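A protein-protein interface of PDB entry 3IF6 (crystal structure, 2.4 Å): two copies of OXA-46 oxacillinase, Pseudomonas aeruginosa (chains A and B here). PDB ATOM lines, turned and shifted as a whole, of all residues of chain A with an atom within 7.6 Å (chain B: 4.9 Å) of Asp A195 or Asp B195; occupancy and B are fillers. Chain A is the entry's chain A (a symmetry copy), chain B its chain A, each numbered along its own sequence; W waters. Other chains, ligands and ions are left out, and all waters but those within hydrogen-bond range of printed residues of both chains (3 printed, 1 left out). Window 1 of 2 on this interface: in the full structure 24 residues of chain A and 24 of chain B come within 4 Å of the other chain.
The side-chain carboxylate (OE1) of Glu A225 lies within salt-bridge range of the guanidinium group (NH1) of Arg B114, 3.9 Å away. NH2 of Arg B191 is in salt-bridge range of OE1 of Glu A91, at 2.7 Å. NH1 of Arg A208 lies within salt-bridge range of OD2 of Asp B195, 3.1 Å away. The side-chain carboxylate (OD2) of Asp A195 is in salt-bridge range of the guanidinium group (NH1) of Arg B208 (3.1 Å). The side-chain carboxylate (OD1) of Asp B195 sits close to the side-chain carboxylate (OD1) of Asp A195, at 3.3 Å.
The side-chain carboxylate (OD2) of Asp B195 is in salt-bridge range of the guanidinium group (NH1) of Arg B114, 2.9 Å away. The guanidinium group of Arg B208 lies within hydrogen-bond range of the backbone carbonyl oxygen of Lys B194 (2.8 Å). The guanidinium group of Arg A114 lies within salt-bridge range of the side-chain carboxylate of Asp A195, 2.9 Å away. O of Trp A223 lies within hydrogen-bond range of N of Arg A208 (2.9 Å). The guanidinium group (NH1) of Arg A208 lies within salt-bridge range of the side-chain carboxylate (OE2) of Glu A225, 3.1 Å away. OE2 of Glu A225 lies within hydrogen-bond range of NE1 of Trp A223 (3.0 Å).
Arg A114 touches Ile B206, and with the chains exchanged Ile A206 touches Arg B114. Arg B191 touches its own counterpart, Arg A191. Asp B195 touches its own counterpart, Asp A195. Ile A198 touches its own counterpart, Ile B198. Positions printed for both chains: 114, 191, 192, 193, 194, 195, 196, 197, 198, 206 and 208. Of the 13 pairs that touch across the chains among the printed residues, 11 have their exchanged pair printed and touching as well.
Of the printed residues of chain B, Glu A91 touches Arg B191 (2.7 Å). Of the printed residues of chain B, Leu A192 touches Arg B191 (3.7 Å). Printed residues of chain B within 4 Å of Asp A195: Asp B195, Ile B206 and Arg B208. Printed residues of chain B within 4 Å of Ile A198: Ile B198 (3.3 Å). Of the printed residues of chain B, Arg A208 touches Asp B195 (2.3 Å). Of the printed residues of chain A, Leu B192 touches Arg A191. Val B193 touches none of the printed residues of chain A. Asp B195 touches just these residues of chain A: Asp A195 (3.3 Å), Ile A206 (3.98 Å) and Arg A208 (2.3 Å). The nearest residue of chain A that does not touch Asp B195 is Ile A198 (4.3 Å).
Of the 11 printed residues of chain B, 7 touch a printed residue of chain A. Hydrophobic or aromatic side chains of chain B within 4 Å of the printed part of chain A: Leu B192, Ile B198 and Ile B206. Among the printed residues, Asp or Glu carboxylates within 4 Å of a Lys or Arg side-chain nitrogen of the other chain: Glu A91 with Arg B191 (2.7 Å), Asp A195 with Arg B208 (2.3 Å), Arg A208 with Asp B195 (2.3 Å) and Glu A225 with Arg B114 (3.9 Å).
CD1 of Ile B206 touches NH2 of Arg A114, at 3.1 Å. Arg A191 touches Arg B191. NH1 of Arg A191 touches CD1 of Leu B192 (3.7 Å). CD1 of Leu A192 touches NH1 of Arg B191 (3.7 Å). OD2 of Asp A195 touches CD1 of Ile B206, 3.98 Å away. CD1 of Ile B198 touches CD1 of Ile A198, 3.3 Å away. Arg B114 touches Ile A206. Ile A206 touches Asp B195.
Water W2 bridges the side-chain carboxylate of Glu A91 (2.7 Å) and the side-chain amino group of Lys B194 (3.0 Å). Water W3 lies within hydrogen-bond range of OD1 of Asp B195 (2.7 Å) and O of Arg A191 (3.0 Å). Water W1 bridges OD1 of Asp A195 (2.7 Å) and O of Arg B191 (3.0 Å).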
ATOM      1  N   GLU A  91      24.343  -9.503   2.529  1.00  0.00           N
ATOM      2  CA  GLU A  91      24.614 -10.454   1.408  1.00  0.00           C
ATOM      3  C   GLU A  91      23.974  -9.956   0.101  1.00  0.00           C
ATOM      4  O   GLU A  91      24.353 -10.376  -0.989  1.00  0.00           O
ATOM      5  CB  GLU A  91      24.047 -11.878   1.627  1.00  0.00           C
ATOM      6  CG  GLU A  91      23.940 -12.389   3.004  1.00  0.00           C
ATOM      7  CD  GLU A  91      22.654 -12.001   3.690  1.00  0.00           C
ATOM      8  OE1 GLU A  91      22.607 -10.887   4.238  1.00  0.00           O
ATOM      9  OE2 GLU A  91      21.721 -12.840   3.729  1.00  0.00           O
ATOM     10  N   ARG A 114      28.997 -12.709  -1.762  1.00  0.00           N
ATOM     11  CA  ARG A 114      29.208 -14.125  -2.045  1.00  0.00           C
ATOM     12  C   ARG A 114      30.043 -14.403  -3.286  1.00  0.00           C
ATOM     13  O   ARG A 114      30.875 -15.306  -3.271  1.00  0.00           O
ATOM     14  CB  ARG A 114      27.890 -14.841  -2.181  1.00  0.00           C
ATOM     15  CG  ARG A 114      28.083 -16.358  -2.066  1.00  0.00           C
ATOM     16  CD  ARG A 114      26.924 -16.905  -1.290  1.00  0.00           C
ATOM     17  NE  ARG A 114      27.406 -17.890  -0.348  1.00  0.00           N
ATOM     18  CZ  ARG A 114      26.877 -18.136   0.841  1.00  0.00           C
ATOM     19  NH1 ARG A 114      25.825 -17.468   1.316  1.00  0.00           N
ATOM     20  NH2 ARG A 114      27.440 -19.079   1.547  1.00  0.00           N
ATOM     21  N   MET A 117      33.599 -13.334  -2.413  1.00  0.00           N
ATOM     22  CA  MET A 117      34.245 -14.375  -1.618  1.00  0.00           C
ATOM     23  C   MET A 117      34.691 -15.553  -2.513  1.00  0.00           C
ATOM     24  O   MET A 117      35.803 -16.105  -2.342  1.00  0.00           O
ATOM     25  CB  MET A 117      33.270 -14.814  -0.523  1.00  0.00           C
ATOM     26  CG  MET A 117      33.797 -15.765   0.541  1.00  0.00           C
ATOM     27  SD  MET A 117      35.230 -15.189   1.448  1.00  0.00           S
ATOM     28  CE  MET A 117      34.465 -14.409   2.869  1.00  0.00           C
ATOM     29  N   ARG A 118      33.845 -15.925  -3.481  1.00  0.00           N
ATOM     30  CA  ARG A 118      34.088 -17.144  -4.249  1.00  0.00           C
ATOM     31  C   ARG A 118      35.031 -16.942  -5.398  1.00  0.00           C
ATOM     32  O   ARG A 118      35.559 -17.927  -5.934  1.00  0.00           O
ATOM     33  CB  ARG A 118      32.788 -17.798  -4.747  1.00  0.00           C
ATOM     34  CG  ARG A 118      31.884 -18.396  -3.665  1.00  0.00           C
ATOM     35  CD  ARG A 118      30.497 -18.673  -4.242  1.00  0.00           C
ATOM     36  NE  ARG A 118      29.652 -19.539  -3.420  1.00  0.00           N
ATOM     37  CZ  ARG A 118      28.371 -19.840  -3.694  1.00  0.00           C
ATOM     38  NH1 ARG A 118      27.736 -19.323  -4.776  1.00  0.00           N
ATOM     39  NH2 ARG A 118      27.696 -20.662  -2.881  1.00  0.00           N
ATOM     40  N   LEU A 178      36.494 -17.331  15.309  1.00  0.00           N
ATOM     41  CA  LEU A 178      35.331 -17.118  14.403  1.00  0.00           C
ATOM     42  C   LEU A 178      34.298 -18.221  14.564  1.00  0.00           C
ATOM     43  O   LEU A 178      33.115 -17.960  14.727  1.00  0.00           O
ATOM     44  CB  LEU A 178      35.792 -17.004  12.938  1.00  0.00           C
ATOM     45  CG  LEU A 178      34.801 -16.940  11.756  1.00  0.00           C
ATOM     46  CD1 LEU A 178      33.905 -15.713  11.797  1.00  0.00           C
ATOM     47  CD2 LEU A 178      35.592 -16.967  10.465  1.00  0.00           C
ATOM     48  N   HIS A 189      27.440 -10.748  11.840  1.00  0.00           N
ATOM     49  CA  HIS A 189      28.494 -10.599  10.840  1.00  0.00           C
ATOM     50  C   HIS A 189      29.385 -11.862  10.775  1.00  0.00           C
ATOM     51  O   HIS A 189      29.812 -12.267   9.686  1.00  0.00           O
ATOM     52  CB  HIS A 189      29.382  -9.366  11.101  1.00  0.00           C
ATOM     53  CG  HIS A 189      28.662  -8.050  11.015  1.00  0.00           C
ATOM     54  ND1 HIS A 189      27.609  -7.819  10.150  1.00  0.00           N
ATOM     55  CD2 HIS A 189      28.888  -6.874  11.645  1.00  0.00           C
ATOM     56  CE1 HIS A 189      27.197  -6.570  10.278  1.00  0.00           C
ATOM     57  NE2 HIS A 189      27.962  -5.974  11.172  1.00  0.00           N
ATOM     58  N   GLN A 190      29.662 -12.449  11.939  1.00  0.00           N
ATOM     59  CA  GLN A 190      30.434 -13.692  12.069  1.00  0.00           C
ATOM     60  C   GLN A 190      29.729 -14.861  11.396  1.00  0.00           C
ATOM     61  O   GLN A 190      30.352 -15.570  10.612  1.00  0.00           O
ATOM     62  CB  GLN A 190      30.769 -13.991  13.545  1.00  0.00           C
ATOM     63  CG  GLN A 190      31.507 -12.807  14.243  1.00  0.00           C
ATOM     64  CD  GLN A 190      32.111 -13.185  15.579  1.00  0.00           C
ATOM     65  OE1 GLN A 190      33.121 -13.867  15.602  1.00  0.00           O
ATOM     66  NE2 GLN A 190      31.503 -12.739  16.703  1.00  0.00           N
ATOM     67  N   ARG A 191      28.442 -15.042  11.697  1.00  0.00           N
ATOM     68  CA  ARG A 191      27.597 -16.023  11.033  1.00  0.00           C
ATOM     69  C   ARG A 191      27.620 -15.828   9.507  1.00  0.00           C
ATOM     70  O   ARG A 191      27.879 -16.775   8.769  1.00  0.00           O
ATOM     71  CB  ARG A 191      26.172 -15.982  11.585  1.00  0.00           C
ATOM     72  CG  ARG A 191      26.084 -16.299  13.105  1.00  0.00           C
ATOM     73  CD  ARG A 191      24.654 -16.617  13.591  1.00  0.00           C
ATOM     74  NE  ARG A 191      24.608 -16.956  15.021  1.00  0.00           N
ATOM     75  CZ  ARG A 191      25.181 -18.029  15.590  1.00  0.00           C
ATOM     76  NH1 ARG A 191      25.823 -18.913  14.853  1.00  0.00           N
ATOM     77  NH2 ARG A 191      25.085 -18.249  16.911  1.00  0.00           N
ATOM     78  N   LEU A 192      27.408 -14.590   9.045  1.00  0.00           N
ATOM     79  CA  LEU A 192      27.424 -14.283   7.613  1.00  0.00           C
ATOM     80  C   LEU A 192      28.708 -14.767   6.939  1.00  0.00           C
ATOM     81  O   LEU A 192      28.665 -15.490   5.915  1.00  0.00           O
ATOM     82  CB  LEU A 192      27.250 -12.771   7.360  1.00  0.00           C
ATOM     83  CG  LEU A 192      27.223 -12.372   5.886  1.00  0.00           C
ATOM     84  CD1 LEU A 192      26.358 -13.370   5.042  1.00  0.00           C
ATOM     85  CD2 LEU A 192      26.746 -10.930   5.692  1.00  0.00           C
ATOM     86  N   VAL A 193      29.833 -14.332   7.488  1.00  0.00           N
ATOM     87  CA  VAL A 193      31.146 -14.690   6.964  1.00  0.00           C
ATOM     88  C   VAL A 193      31.314 -16.193   6.975  1.00  0.00           C
ATOM     89  O   VAL A 193      31.748 -16.755   5.999  1.00  0.00           O
ATOM     90  CB  VAL A 193      32.276 -13.930   7.691  1.00  0.00           C
ATOM     91  CG1 VAL A 193      33.676 -14.498   7.377  1.00  0.00           C
ATOM     92  CG2 VAL A 193      32.204 -12.420   7.315  1.00  0.00           C
ATOM     93  N   LYS A 194      30.885 -16.844   8.049  1.00  0.00           N
ATOM     94  CA  LYS A 194      30.941 -18.289   8.084  1.00  0.00           C
ATOM     95  C   LYS A 194      30.049 -18.960   7.054  1.00  0.00           C
ATOM     96  O   LYS A 194      30.341 -20.049   6.600  1.00  0.00           O
ATOM     97  CB  LYS A 194      30.659 -18.807   9.489  1.00  0.00           C
ATOM     98  CG  LYS A 194      31.838 -18.635  10.459  1.00  0.00           C
ATOM     99  CD  LYS A 194      31.510 -19.272  11.834  1.00  0.00           C
ATOM    100  CE  LYS A 194      30.643 -18.334  12.628  1.00  0.00           C
ATOM    101  NZ  LYS A 194      30.198 -19.000  13.868  1.00  0.00           N
ATOM    102  N   ASP A 195      28.957 -18.305   6.688  1.00  0.00           N
ATOM    103  CA  ASP A 195      28.089 -18.802   5.627  1.00  0.00           C
ATOM    104  C   ASP A 195      28.790 -18.545   4.262  1.00  0.00           C
ATOM    105  O   ASP A 195      28.748 -19.398   3.365  1.00  0.00           O
ATOM    106  CB  ASP A 195      26.680 -18.202   5.753  1.00  0.00           C
ATOM    107  CG  ASP A 195      25.591 -19.062   5.071  1.00  0.00           C
ATOM    108  OD1 ASP A 195      24.881 -19.919   5.771  1.00  0.00           O
ATOM    109  OD2 ASP A 195      25.445 -18.855   3.839  1.00  0.00           O
ATOM    110  N   LEU A 196      29.501 -17.439   4.124  1.00  0.00           N
ATOM    111  CA  LEU A 196      30.195 -17.153   2.853  1.00  0.00           C
ATOM    112  C   LEU A 196      31.335 -18.113   2.512  1.00  0.00           C
ATOM    113  O   LEU A 196      31.779 -18.164   1.371  1.00  0.00           O
ATOM    114  CB  LEU A 196      30.720 -15.704   2.797  1.00  0.00           C
ATOM    115  CG  LEU A 196      29.724 -14.532   2.981  1.00  0.00           C
ATOM    116  CD1 LEU A 196      30.503 -13.213   3.112  1.00  0.00           C
ATOM    117  CD2 LEU A 196      28.697 -14.461   1.801  1.00  0.00           C
ATOM    118  N   MET A 197      31.803 -18.847   3.516  1.00  0.00           N
ATOM    119  CA  MET A 197      32.985 -19.655   3.433  1.00  0.00           C
ATOM    120  C   MET A 197      32.632 -21.083   3.051  1.00  0.00           C
ATOM    121  O   MET A 197      33.531 -21.878   2.818  1.00  0.00           O
ATOM    122  CB  MET A 197      33.675 -19.682   4.788  1.00  0.00           C
ATOM    123  CG  MET A 197      34.573 -18.491   5.099  1.00  0.00           C
ATOM    124  SD  MET A 197      34.968 -18.557   6.880  1.00  0.00           S
ATOM    125  CE  MET A 197      36.265 -19.813   6.905  1.00  0.00           C
ATOM    126  N   ILE A 198      31.348 -21.422   3.031  1.00  0.00           N
ATOM    127  CA  ILE A 198      30.926 -22.749   2.609  1.00  0.00           C
ATOM    128  C   ILE A 198      31.360 -23.066   1.175  1.00  0.00           C
ATOM    129  O   ILE A 198      30.978 -22.378   0.222  1.00  0.00           O
ATOM    130  CB  ILE A 198      29.404 -22.930   2.738  1.00  0.00           C
ATOM    131  CG1 ILE A 198      28.973 -22.643   4.181  1.00  0.00           C
ATOM    132  CG2 ILE A 198      28.979 -24.355   2.229  1.00  0.00           C
ATOM    133  CD1 ILE A 198      27.486 -22.766   4.465  1.00  0.00           C
ATOM    134  N   THR A 199      32.192 -24.100   1.035  1.00  0.00           N
ATOM    135  CA  THR A 199      32.544 -24.634  -0.295  1.00  0.00           C
ATOM    136  C   THR A 199      31.800 -25.956  -0.594  1.00  0.00           C
ATOM    137  O   THR A 199      31.696 -26.342  -1.735  1.00  0.00           O
ATOM    138  CB  THR A 199      34.098 -24.786  -0.487  1.00  0.00           C
ATOM    139  OG1 THR A 199      34.631 -25.671   0.496  1.00  0.00           O
ATOM    140  CG2 THR A 199      34.833 -23.415  -0.359  1.00  0.00           C
ATOM    141  N   ILE A 206      29.768 -29.907   7.139  1.00  0.00           N
ATOM    142  CA  ILE A 206      29.907 -28.643   6.404  1.00  0.00           C
ATOM    143  C   ILE A 206      31.359 -28.274   6.281  1.00  0.00           C
ATOM    144  O   ILE A 206      32.048 -28.148   7.304  1.00  0.00           O
ATOM    145  CB  ILE A 206      29.114 -27.476   7.077  1.00  0.00           C
ATOM    146  CG1 ILE A 206      27.648 -27.890   7.326  1.00  0.00           C
ATOM    147  CG2 ILE A 206      29.174 -26.233   6.231  1.00  0.00           C
ATOM    148  CD1 ILE A 206      26.800 -26.764   7.927  1.00  0.00           C
ATOM    149  N   LEU A 207      31.816 -28.052   5.045  1.00  0.00           N
ATOM    150  CA  LEU A 207      33.168 -27.617   4.800  1.00  0.00           C
ATOM    151  C   LEU A 207      33.158 -26.121   4.527  1.00  0.00           C
ATOM    152  O   LEU A 207      32.411 -25.676   3.660  1.00  0.00           O
ATOM    153  CB  LEU A 207      33.779 -28.435   3.640  1.00  0.00           C
ATOM    154  CG  LEU A 207      35.060 -27.970   2.977  1.00  0.00           C
ATOM    155  CD1 LEU A 207      36.112 -27.853   4.031  1.00  0.00           C
ATOM    156  CD2 LEU A 207      35.480 -28.950   1.933  1.00  0.00           C
ATOM    157  N   ARG A 208      33.950 -25.341   5.283  1.00  0.00           N
ATOM    158  CA  ARG A 208      33.993 -23.852   5.168  1.00  0.00           C
ATOM    159  C   ARG A 208      35.468 -23.481   5.012  1.00  0.00           C
ATOM    160  O   ARG A 208      36.232 -23.713   5.944  1.00  0.00           O
ATOM    161  CB  ARG A 208      33.391 -23.141   6.418  1.00  0.00           C
ATOM    162  CG  ARG A 208      32.216 -23.833   7.035  1.00  0.00           C
ATOM    163  CD  ARG A 208      31.622 -23.224   8.356  1.00  0.00           C
ATOM    164  NE  ARG A 208      30.422 -22.547   7.953  1.00  0.00           N
ATOM    165  CZ  ARG A 208      29.165 -22.758   8.312  1.00  0.00           C
ATOM    166  NH1 ARG A 208      28.789 -23.607   9.275  1.00  0.00           N
ATOM    167  NH2 ARG A 208      28.252 -22.005   7.681  1.00  0.00           N
ATOM    168  N   TRP A 223      37.698 -25.084   8.073  1.00  0.00           N
ATOM    169  CA  TRP A 223      37.405 -26.260   8.881  1.00  0.00           C
ATOM    170  C   TRP A 223      36.282 -27.040   8.215  1.00  0.00           C
ATOM    171  O   TRP A 223      35.687 -26.587   7.251  1.00  0.00           O
ATOM    172  CB  TRP A 223      37.056 -25.886  10.322  1.00  0.00           C
ATOM    173  CG  TRP A 223      35.855 -25.066  10.531  1.00  0.00           C
ATOM    174  CD1 TRP A 223      34.576 -25.522  10.732  1.00  0.00           C
ATOM    175  CD2 TRP A 223      35.779 -23.614  10.616  1.00  0.00           C
ATOM    176  NE1 TRP A 223      33.714 -24.457  10.900  1.00  0.00           N
ATOM    177  CE2 TRP A 223      34.427 -23.282  10.851  1.00  0.00           C
ATOM    178  CE3 TRP A 223      36.719 -22.583  10.501  1.00  0.00           C
ATOM    179  CZ2 TRP A 223      33.990 -21.955  10.978  1.00  0.00           C
ATOM    180  CZ3 TRP A 223      36.303 -21.284  10.628  1.00  0.00           C
ATOM    181  CH2 TRP A 223      34.934 -20.976  10.860  1.00  0.00           C
ATOM    182  N   GLU A 225      32.947 -29.248   9.858  1.00  0.00           N
ATOM    183  CA  GLU A 225      32.183 -29.561  11.055  1.00  0.00           C
ATOM    184  C   GLU A 225      31.547 -30.917  10.929  1.00  0.00           C
ATOM    185  O   GLU A 225      31.041 -31.244   9.870  1.00  0.00           O
ATOM    186  CB  GLU A 225      31.066 -28.567  11.208  1.00  0.00           C
ATOM    187  CG  GLU A 225      31.551 -27.142  11.238  1.00  0.00           C
ATOM    188  CD  GLU A 225      30.440 -26.132  11.310  1.00  0.00           C
ATOM    189  OE1 GLU A 225      29.262 -26.493  11.409  1.00  0.00           O
ATOM    190  OE2 GLU A 225      30.776 -24.956  11.290  1.00  0.00           O
ATOM    191  N   ARG B 114      21.877 -28.386  16.256  1.00  0.00           N
ATOM    192  CA  ARG B 114      22.133 -29.001  14.958  1.00  0.00           C
ATOM    193  C   ARG B 114      21.697 -30.454  14.850  1.00  0.00           C
ATOM    194  O   ARG B 114      21.164 -30.855  13.818  1.00  0.00           O
ATOM    195  CB  ARG B 114      23.595 -28.910  14.607  1.00  0.00           C
ATOM    196  CG  ARG B 114      23.810 -29.166  13.110  1.00  0.00           C
ATOM    197  CD  ARG B 114      24.879 -28.228  12.639  1.00  0.00           C
ATOM    198  NE  ARG B 114      24.497 -27.679  11.357  1.00  0.00           N
ATOM    199  CZ  ARG B 114      24.804 -26.467  10.921  1.00  0.00           C
ATOM    200  NH1 ARG B 114      25.501 -25.593  11.647  1.00  0.00           N
ATOM    201  NH2 ARG B 114      24.386 -26.154   9.725  1.00  0.00           N
ATOM    202  N   ARG B 191      20.137 -16.076  10.572  1.00  0.00           N
ATOM    203  CA  ARG B 191      21.343 -16.666  10.012  1.00  0.00           C
ATOM    204  C   ARG B 191      21.597 -18.065  10.600  1.00  0.00           C
ATOM    205  O   ARG B 191      21.777 -19.023   9.853  1.00  0.00           O
ATOM    206  CB  ARG B 191      22.547 -15.745  10.210  1.00  0.00           C
ATOM    207  CG  ARG B 191      22.388 -14.358   9.523  1.00  0.00           C
ATOM    208  CD  ARG B 191      23.711 -13.571   9.403  1.00  0.00           C
ATOM    209  NE  ARG B 191      23.539 -12.285   8.711  1.00  0.00           N
ATOM    210  CZ  ARG B 191      23.177 -12.129   7.427  1.00  0.00           C
ATOM    211  NH1 ARG B 191      22.980 -13.180   6.657  1.00  0.00           N
ATOM    212  NH2 ARG B 191      23.043 -10.908   6.886  1.00  0.00           N
ATOM    213  N   LEU B 192      21.553 -18.187  11.932  1.00  0.00           N
ATOM    214  CA  LEU B 192      21.761 -19.472  12.601  1.00  0.00           C
ATOM    215  C   LEU B 192      20.839 -20.559  12.051  1.00  0.00           C
ATOM    216  O   LEU B 192      21.301 -21.658  11.656  1.00  0.00           O
ATOM    217  CB  LEU B 192      21.560 -19.352  14.126  1.00  0.00           C
ATOM    218  CG  LEU B 192      21.793 -20.646  14.903  1.00  0.00           C
ATOM    219  CD1 LEU B 192      23.061 -21.403  14.379  1.00  0.00           C
ATOM    220  CD2 LEU B 192      21.882 -20.402  16.411  1.00  0.00           C
ATOM    221  N   VAL B 193      19.547 -20.267  12.068  1.00  0.00           N
ATOM    222  CA  VAL B 193      18.529 -21.196  11.590  1.00  0.00           C
ATOM    223  C   VAL B 193      18.787 -21.541  10.140  1.00  0.00           C
ATOM    224  O   VAL B 193      18.747 -22.692   9.780  1.00  0.00           O
ATOM    225  CB  VAL B 193      17.105 -20.671  11.864  1.00  0.00           C
ATOM    226  CG1 VAL B 193      16.019 -21.470  11.112  1.00  0.00           C
ATOM    227  CG2 VAL B 193      16.834 -20.696  13.398  1.00  0.00           C
ATOM    228  N   LYS B 194      19.137 -20.547   9.333  1.00  0.00           N
ATOM    229  CA  LYS B 194      19.477 -20.826   7.954  1.00  0.00           C
ATOM    230  C   LYS B 194      20.721 -21.682   7.794  1.00  0.00           C
ATOM    231  O   LYS B 194      20.847 -22.413   6.831  1.00  0.00           O
ATOM    232  CB  LYS B 194      19.582 -19.535   7.152  1.00  0.00           C
ATOM    233  CG  LYS B 194      18.220 -18.916   6.799  1.00  0.00           C
ATOM    234  CD  LYS B 194      18.407 -17.664   5.902  1.00  0.00           C
ATOM    235  CE  LYS B 194      18.787 -16.486   6.756  1.00  0.00           C
ATOM    236  NZ  LYS B 194      19.121 -15.335   5.894  1.00  0.00           N
ATOM    237  N   ASP B 195      21.641 -21.589   8.743  1.00  0.00           N
ATOM    238  CA  ASP B 195      22.821 -22.446   8.749  1.00  0.00           C
ATOM    239  C   ASP B 195      22.388 -23.869   9.206  1.00  0.00           C
ATOM    240  O   ASP B 195      22.858 -24.875   8.654  1.00  0.00           O
ATOM    241  CB  ASP B 195      23.946 -21.815   9.582  1.00  0.00           C
ATOM    242  CG  ASP B 195      25.351 -22.329   9.194  1.00  0.00           C
ATOM    243  OD1 ASP B 195      26.103 -21.651   8.354  1.00  0.00           O
ATOM    244  OD2 ASP B 195      25.696 -23.403   9.750  1.00  0.00           O
ATOM    245  N   LEU B 196      21.446 -23.970  10.127  1.00  0.00           N
ATOM    246  CA  LEU B 196      20.991 -25.296  10.587  1.00  0.00           C
ATOM    247  C   LEU B 196      20.263 -26.129   9.531  1.00  0.00           C
ATOM    248  O   LEU B 196      20.108 -27.334   9.694  1.00  0.00           O
ATOM    249  CB  LEU B 196      20.110 -25.198  11.849  1.00  0.00           C
ATOM    250  CG  LEU B 196      20.678 -24.509  13.115  1.00  0.00           C
ATOM    251  CD1 LEU B 196      19.554 -24.332  14.149  1.00  0.00           C
ATOM    252  CD2 LEU B 196      21.875 -25.317  13.720  1.00  0.00           C
ATOM    253  N   MET B 197      19.812 -25.467   8.471  1.00  0.00           N
ATOM    254  CA  MET B 197      18.946 -26.037   7.480  1.00  0.00           C
ATOM    255  C   MET B 197      19.755 -26.591   6.318  1.00  0.00           C
ATOM    256  O   MET B 197      19.184 -27.221   5.440  1.00  0.00           O
ATOM    257  CB  MET B 197      18.015 -24.963   6.942  1.00  0.00           C
ATOM    258  CG  MET B 197      16.778 -24.675   7.782  1.00  0.00           C
ATOM    259  SD  MET B 197      16.041 -23.127   7.156  1.00  0.00           S
ATOM    260  CE  MET B 197      15.169 -23.720   5.691  1.00  0.00           C
ATOM    261  N   ILE B 198      21.056 -26.324   6.282  1.00  0.00           N
ATOM    262  CA  ILE B 198      21.910 -26.874   5.241  1.00  0.00           C
ATOM    263  C   ILE B 198      21.901 -28.405   5.235  1.00  0.00           C
ATOM    264  O   ILE B 198      22.274 -29.053   6.219  1.00  0.00           O
ATOM    265  CB  ILE B 198      23.357 -26.368   5.366  1.00  0.00           C
ATOM    266  CG1 ILE B 198      23.370 -24.835   5.340  1.00  0.00           C
ATOM    267  CG2 ILE B 198      24.259 -27.020   4.256  1.00  0.00           C
ATOM    268  CD1 ILE B 198      24.734 -24.182   5.470  1.00  0.00           C
ATOM    269  N   ILE B 206      24.000 -23.767  -2.445  1.00  0.00           N
ATOM    270  CA  ILE B 206      23.678 -24.236  -1.090  1.00  0.00           C
ATOM    271  C   ILE B 206      22.243 -24.678  -1.024  1.00  0.00           C
ATOM    272  O   ILE B 206      21.342 -23.883  -1.330  1.00  0.00           O
ATOM    273  CB  ILE B 206      23.952 -23.146  -0.005  1.00  0.00           C
ATOM    274  CG1 ILE B 206      25.385 -22.591  -0.144  1.00  0.00           C
ATOM    275  CG2 ILE B 206      23.734 -23.702   1.377  1.00  0.00           C
ATOM    276  CD1 ILE B 206      25.737 -21.561   0.935  1.00  0.00           C
ATOM    277  N   ARG B 208      19.219 -25.733   1.437  1.00  0.00           N
ATOM    278  CA  ARG B 208      18.792 -25.548   2.856  1.00  0.00           C
ATOM    279  C   ARG B 208      17.342 -26.027   2.928  1.00  0.00           C
ATOM    280  O   ARG B 208      16.489 -25.411   2.295  1.00  0.00           O
ATOM    281  CB  ARG B 208      18.888 -24.062   3.318  1.00  0.00           C
ATOM    282  CG  ARG B 208      20.047 -23.299   2.756  1.00  0.00           C
ATOM    283  CD  ARG B 208      20.149 -21.769   3.101  1.00  0.00           C
ATOM    284  NE  ARG B 208      21.172 -21.676   4.104  1.00  0.00           N
ATOM    285  CZ  ARG B 208      22.330 -21.034   4.082  1.00  0.00           C
ATOM    286  NH1 ARG B 208      22.709 -20.200   3.107  1.00  0.00           N
ATOM    287  NH2 ARG B 208      23.112 -21.219   5.155  1.00  0.00           N
HETATM  288  O   HOH W   1      23.763 -18.356   7.722  1.00  0.00           O
HETATM  289  O   HOH W   2      20.032 -14.797   3.056  1.00  0.00           O
HETATM  290  O   HOH W   3      26.294 -19.189   9.538  1.00  0.00           O
